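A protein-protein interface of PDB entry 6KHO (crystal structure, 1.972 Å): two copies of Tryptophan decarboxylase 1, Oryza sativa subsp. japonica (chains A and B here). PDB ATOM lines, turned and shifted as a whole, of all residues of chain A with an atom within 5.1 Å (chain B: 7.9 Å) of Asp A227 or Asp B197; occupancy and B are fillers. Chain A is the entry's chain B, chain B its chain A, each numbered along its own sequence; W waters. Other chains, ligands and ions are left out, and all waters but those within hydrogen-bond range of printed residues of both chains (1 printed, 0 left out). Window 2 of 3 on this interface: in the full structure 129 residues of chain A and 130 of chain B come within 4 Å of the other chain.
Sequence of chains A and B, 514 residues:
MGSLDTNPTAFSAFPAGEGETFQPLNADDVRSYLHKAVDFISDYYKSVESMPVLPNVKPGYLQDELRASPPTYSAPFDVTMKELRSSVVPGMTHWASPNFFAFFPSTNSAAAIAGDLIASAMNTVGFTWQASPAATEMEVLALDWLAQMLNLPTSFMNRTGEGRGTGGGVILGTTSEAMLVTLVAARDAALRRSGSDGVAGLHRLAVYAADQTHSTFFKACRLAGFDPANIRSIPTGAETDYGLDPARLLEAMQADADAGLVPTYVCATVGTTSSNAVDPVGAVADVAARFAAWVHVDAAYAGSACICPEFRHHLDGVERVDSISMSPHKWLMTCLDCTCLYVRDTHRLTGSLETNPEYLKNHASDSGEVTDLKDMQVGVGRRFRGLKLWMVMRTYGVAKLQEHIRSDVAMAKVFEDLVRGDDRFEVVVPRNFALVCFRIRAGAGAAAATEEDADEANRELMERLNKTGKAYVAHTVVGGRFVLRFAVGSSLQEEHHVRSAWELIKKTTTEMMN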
ATOM      1  N   HIS A 203      19.060   8.000 -15.203  1.00  0.00           N
ATOM      2  CA  HIS A 203      19.156   6.748 -15.952  1.00  0.00           C
ATOM      3  C   HIS A 203      19.745   5.598 -15.142  1.00  0.00           C
ATOM      4  O   HIS A 203      19.737   4.462 -15.626  1.00  0.00           O
ATOM      5  CB  HIS A 203      20.002   6.964 -17.210  1.00  0.00           C
ATOM      6  CG  HIS A 203      21.459   7.135 -16.914  1.00  0.00           C
ATOM      7  ND1 HIS A 203      21.985   8.321 -16.442  1.00  0.00           N
ATOM      8  CD2 HIS A 203      22.492   6.265 -16.985  1.00  0.00           C
ATOM      9  CE1 HIS A 203      23.284   8.176 -16.253  1.00  0.00           C
ATOM     10  NE2 HIS A 203      23.616   6.937 -16.571  1.00  0.00           N
ATOM     11  N   LEU A 205      18.465   4.871 -12.013  1.00  0.00           N
ATOM     12  CA  LEU A 205      17.463   4.457 -11.024  1.00  0.00           C
ATOM     13  C   LEU A 205      16.605   3.307 -11.545  1.00  0.00           C
ATOM     14  O   LEU A 205      16.089   3.364 -12.666  1.00  0.00           O
ATOM     15  CB  LEU A 205      16.571   5.641 -10.639  1.00  0.00           C
ATOM     16  CG  LEU A 205      17.227   6.925 -10.118  1.00  0.00           C
ATOM     17  CD1 LEU A 205      16.170   7.870  -9.514  1.00  0.00           C
ATOM     18  CD2 LEU A 205      18.314   6.620  -9.096  1.00  0.00           C
ATOM     19  N   GLY A 225       9.757   9.685 -15.413  1.00  0.00           N
ATOM     20  CA  GLY A 225      11.044   9.786 -16.082  1.00  0.00           C
ATOM     21  C   GLY A 225      11.989   8.627 -15.868  1.00  0.00           C
ATOM     22  O   GLY A 225      13.156   8.717 -16.286  1.00  0.00           O
ATOM     23  N   PHE A 226      11.540   7.554 -15.223  1.00  0.00           N
ATOM     24  CA  PHE A 226      12.364   6.363 -15.108  1.00  0.00           C
ATOM     25  C   PHE A 226      12.596   5.752 -16.488  1.00  0.00           C
ATOM     26  O   PHE A 226      11.724   5.799 -17.361  1.00  0.00           O
ATOM     27  CB  PHE A 226      11.710   5.344 -14.180  1.00  0.00           C
ATOM     28  CG  PHE A 226      11.752   5.738 -12.729  1.00  0.00           C
ATOM     29  CD1 PHE A 226      12.888   5.507 -11.969  1.00  0.00           C
ATOM     30  CD2 PHE A 226      10.662   6.356 -12.128  1.00  0.00           C
ATOM     31  CE1 PHE A 226      12.926   5.868 -10.627  1.00  0.00           C
ATOM     32  CE2 PHE A 226      10.694   6.707 -10.788  1.00  0.00           C
ATOM     33  CZ  PHE A 226      11.826   6.472 -10.037  1.00  0.00           C
ATOM     34  N   ASP A 227      13.795   5.195 -16.672  1.00  0.00           N
ATOM     35  CA  ASP A 227      14.181   4.595 -17.938  1.00  0.00           C
ATOM     36  C   ASP A 227      13.414   3.301 -18.160  1.00  0.00           C
ATOM     37  O   ASP A 227      13.413   2.441 -17.278  1.00  0.00           O
ATOM     38  CB  ASP A 227      15.691   4.306 -17.937  1.00  0.00           C
ATOM     39  CG  ASP A 227      16.250   4.089 -19.328  1.00  0.00           C
ATOM     40  OD1 ASP A 227      15.766   3.169 -20.031  1.00  0.00           O
ATOM     41  OD2 ASP A 227      17.176   4.838 -19.715  1.00  0.00           O
ATOM     42  N   PRO A 228      12.771   3.116 -19.321  1.00  0.00           N
ATOM     43  CA  PRO A 228      12.107   1.833 -19.601  1.00  0.00           C
ATOM     44  C   PRO A 228      12.980   0.613 -19.359  1.00  0.00           C
ATOM     45  O   PRO A 228      12.475  -0.419 -18.904  1.00  0.00           O
ATOM     46  CB  PRO A 228      11.723   1.976 -21.082  1.00  0.00           C
ATOM     47  CG  PRO A 228      11.475   3.425 -21.239  1.00  0.00           C
ATOM     48  CD  PRO A 228      12.532   4.098 -20.394  1.00  0.00           C
ATOM     49  N   ALA A 229      14.284   0.710 -19.631  1.00  0.00           N
ATOM     50  CA  ALA A 229      15.201  -0.402 -19.406  1.00  0.00           C
ATOM     51  C   ALA A 229      15.344  -0.758 -17.935  1.00  0.00           C
ATOM     52  O   ALA A 229      15.801  -1.864 -17.626  1.00  0.00           O
ATOM     53  CB  ALA A 229      16.585  -0.067 -19.986  1.00  0.00           C
ATOM     54  N   ASN A 230      14.975   0.148 -17.024  1.00  0.00           N
ATOM     55  CA  ASN A 230      15.161  -0.053 -15.591  1.00  0.00           C
ATOM     56  C   ASN A 230      13.845  -0.251 -14.846  1.00  0.00           C
ATOM     57  O   ASN A 230      13.834  -0.242 -13.609  1.00  0.00           O
ATOM     58  CB  ASN A 230      15.929   1.125 -14.986  1.00  0.00           C
ATOM     59  CG  ASN A 230      17.321   1.276 -15.584  1.00  0.00           C
ATOM     60  OD1 ASN A 230      17.857   0.338 -16.177  1.00  0.00           O
ATOM     61  ND2 ASN A 230      17.905   2.451 -15.429  1.00  0.00           N
ATOM     62  N   ILE A 231      12.745  -0.437 -15.563  1.00  0.00           N
ATOM     63  CA  ILE A 231      11.434  -0.669 -14.962  1.00  0.00           C
ATOM     64  C   ILE A 231      11.187  -2.169 -14.980  1.00  0.00           C
ATOM     65  O   ILE A 231      10.958  -2.759 -16.043  1.00  0.00           O
ATOM     66  CB  ILE A 231      10.341   0.110 -15.705  1.00  0.00           C
ATOM     67  CG1 ILE A 231      10.641   1.602 -15.596  1.00  0.00           C
ATOM     68  CG2 ILE A 231       8.955  -0.226 -15.145  1.00  0.00           C
ATOM     69  CD1 ILE A 231       9.774   2.477 -16.469  1.00  0.00           C
ATOM     70  N   LEU B 191      13.145  13.423 -26.550  1.00  0.00           N
ATOM     71  CA  LEU B 191      14.105  12.355 -26.276  1.00  0.00           C
ATOM     72  C   LEU B 191      14.275  11.432 -27.477  1.00  0.00           C
ATOM     73  O   LEU B 191      15.390  11.023 -27.808  1.00  0.00           O
ATOM     74  CB  LEU B 191      13.653  11.543 -25.063  1.00  0.00           C
ATOM     75  CG  LEU B 191      13.708  12.232 -23.696  1.00  0.00           C
ATOM     76  CD1 LEU B 191      13.141  11.293 -22.601  1.00  0.00           C
ATOM     77  CD2 LEU B 191      15.136  12.690 -23.384  1.00  0.00           C
ATOM     78  N   SER B 194      16.065  13.437 -30.505  1.00  0.00           N
ATOM     79  CA  SER B 194      17.421  13.886 -30.199  1.00  0.00           C
ATOM     80  C   SER B 194      18.380  12.737 -29.915  1.00  0.00           C
ATOM     81  O   SER B 194      19.570  12.979 -29.705  1.00  0.00           O
ATOM     82  CB  SER B 194      17.411  14.859 -29.014  1.00  0.00           C
ATOM     83  OG  SER B 194      17.186  14.179 -27.792  1.00  0.00           O
ATOM     84  N   GLY B 195      17.907  11.498 -29.919  1.00  0.00           N
ATOM     85  CA  GLY B 195      18.809  10.379 -29.747  1.00  0.00           C
ATOM     86  C   GLY B 195      19.261  10.140 -28.323  1.00  0.00           C
ATOM     87  O   GLY B 195      20.388   9.679 -28.105  1.00  0.00           O
ATOM     88  N   SER B 196      18.419  10.454 -27.343  1.00  0.00           N
ATOM     89  CA  SER B 196      18.735  10.122 -25.961  1.00  0.00           C
ATOM     90  C   SER B 196      18.929   8.613 -25.818  1.00  0.00           C
ATOM     91  O   SER B 196      18.238   7.815 -26.460  1.00  0.00           O
ATOM     92  CB  SER B 196      17.605  10.613 -25.041  1.00  0.00           C
ATOM     93  OG  SER B 196      17.732  10.116 -23.715  1.00  0.00           O
ATOM     94  N   ASP B 197      19.899   8.218 -24.995  1.00  0.00           N
ATOM     95  CA  ASP B 197      20.084   6.810 -24.643  1.00  0.00           C
ATOM     96  C   ASP B 197      19.154   6.533 -23.465  1.00  0.00           C
ATOM     97  O   ASP B 197      19.508   6.739 -22.302  1.00  0.00           O
ATOM     98  CB  ASP B 197      21.544   6.511 -24.307  1.00  0.00           C
ATOM     99  CG  ASP B 197      22.513   6.833 -25.467  1.00  0.00           C
ATOM    100  OD1 ASP B 197      22.192   6.524 -26.641  1.00  0.00           O
ATOM    101  OD2 ASP B 197      23.608   7.383 -25.199  1.00  0.00           O
ATOM    102  N   GLY B 198      17.938   6.074 -23.765  1.00  0.00           N
ATOM    103  CA  GLY B 198      16.934   5.962 -22.717  1.00  0.00           C
ATOM    104  C   GLY B 198      16.600   7.348 -22.195  1.00  0.00           C
ATOM    105  O   GLY B 198      16.315   8.262 -22.975  1.00  0.00           O
ATOM    106  N   VAL B 199      16.646   7.530 -20.872  1.00  0.00           N
ATOM    107  CA  VAL B 199      16.452   8.852 -20.281  1.00  0.00           C
ATOM    108  C   VAL B 199      17.779   9.519 -19.920  1.00  0.00           C
ATOM    109  O   VAL B 199      17.781  10.557 -19.249  1.00  0.00           O
ATOM    110  CB  VAL B 199      15.512   8.808 -19.059  1.00  0.00           C
ATOM    111  CG1 VAL B 199      14.174   8.183 -19.434  1.00  0.00           C
ATOM    112  CG2 VAL B 199      16.152   8.067 -17.894  1.00  0.00           C
ATOM    113  N   ALA B 200      18.912   8.948 -20.349  1.00  0.00           N
ATOM    114  CA  ALA B 200      20.198   9.603 -20.104  1.00  0.00           C
ATOM    115  C   ALA B 200      20.216  11.024 -20.655  1.00  0.00           C
ATOM    116  O   ALA B 200      20.903  11.893 -20.106  1.00  0.00           O
ATOM    117  CB  ALA B 200      21.343   8.784 -20.707  1.00  0.00           C
ATOM    118  N   GLY B 201      19.455  11.286 -21.718  1.00  0.00           N
ATOM    119  CA  GLY B 201      19.394  12.594 -22.331  1.00  0.00           C
ATOM    120  C   GLY B 201      18.420  13.569 -21.714  1.00  0.00           C
ATOM    121  O   GLY B 201      18.324  14.700 -22.198  1.00  0.00           O
ATOM    122  N   LEU B 202      17.698  13.179 -20.656  1.00  0.00           N
ATOM    123  CA  LEU B 202      16.687  14.066 -20.077  1.00  0.00           C
ATOM    124  C   LEU B 202      17.303  15.348 -19.526  1.00  0.00           C
ATOM    125  O   LEU B 202      16.677  16.416 -19.590  1.00  0.00           O
ATOM    126  CB  LEU B 202      15.898  13.327 -18.985  1.00  0.00           C
ATOM    127  CG  LEU B 202      14.644  13.960 -18.360  1.00  0.00           C
ATOM    128  CD1 LEU B 202      13.873  14.836 -19.337  1.00  0.00           C
ATOM    129  CD2 LEU B 202      13.697  12.889 -17.783  1.00  0.00           C
ATOM    130  N   ARG B 204      19.330  17.233 -20.781  1.00  0.00           N
ATOM    131  CA  ARG B 204      19.595  18.208 -21.824  1.00  0.00           C
ATOM    132  C   ARG B 204      18.344  18.901 -22.353  1.00  0.00           C
ATOM    133  O   ARG B 204      18.469  19.822 -23.165  1.00  0.00           O
ATOM    134  CB  ARG B 204      20.342  17.544 -22.986  1.00  0.00           C
ATOM    135  CG  ARG B 204      21.781  17.163 -22.644  1.00  0.00           C
ATOM    136  CD  ARG B 204      22.615  16.900 -23.900  1.00  0.00           C
ATOM    137  NE  ARG B 204      21.939  16.012 -24.849  1.00  0.00           N
ATOM    138  CZ  ARG B 204      21.492  16.381 -26.052  1.00  0.00           C
ATOM    139  NH1 ARG B 204      21.648  17.631 -26.475  1.00  0.00           N
ATOM    140  NH2 ARG B 204      20.892  15.497 -26.844  1.00  0.00           N
HETATM  141  O   HOH W   1      19.798  10.322 -16.864  1.00  0.00           O
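Water W1 lies within hydrogen-bond range of the backbone NH of His A203 and the backbone carbonyl oxygen of Val B199.
No position is printed for both chains.
Printed residues of chain B that touch a printed residue of chain A: Asp B197, Gly B198, Val B199 and Ala B200.
Hydrophobic or aromatic side chains of chain B within 4 Å of the printed part of chain A: Val B199.
Of the 9 printed residues of chain A, 4 touch a printed residue of chain B.
Hydrophobic or aromatic side chains of chain A within 4 Å of the printed part of chain B: His A203.
Of the printed residues of chain A, Asp B197 touches Asp A227 (3.97 Å).
No residue of chain B comes within 4 Å of Pro A228.
Of the printed residues of chain A, Val B199 touches His A203, Gly A225, Phe A226 and Asp A227.
Printed residues of chain A within 4 Å of Gly B198: Asp A227 (3.2 Å).
Of the printed residues of chain B, Phe A226 touches Val B199.
Leu A205 touches none of the printed residues of chain B.
Ile A231 touches none of the printed residues of chain B.
The nearest residue of chain B that does not touch Asp A227 is Ala B200 (4.5 Å).
The nearest printed residue of chain A that does not touch Asp B197 is His A203 (5.1 Å).
The nearest printed residue of chain A that does not touch Ala B200 is Asp A227 (4.5 Å).
Val B199 touches His A203.
His A203 touches Ala B200.
CG1 of Val B199 touches O of Gly A225 (3.4 Å).
Phe A226 touches Val B199 (O to CG1, 3.998 Å).
Asp A227 touches Asp B197 (OD2 to O, 3.97 Å).
Asp A227 touches Gly B198 (OD2 to CA, 3.2 Å).
The side-chain carboxylate (OD2) of Asp A227 lies within hydrogen-bond range of the backbone NH (N) of Val B199, 3.0 Å away.
The backbone carbonyl oxygen of Gly B198 sits at hydrogen-bond distance from the side-chain hydroxyl of Ser B196 (2.4 Å).
O of His A203 sits at hydrogen-bond distance from ND2 of Asn A230 (2.7 Å).
OD1 of Asp A227 sits at hydrogen-bond distance from N of Ala A229 (2.9 Å).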
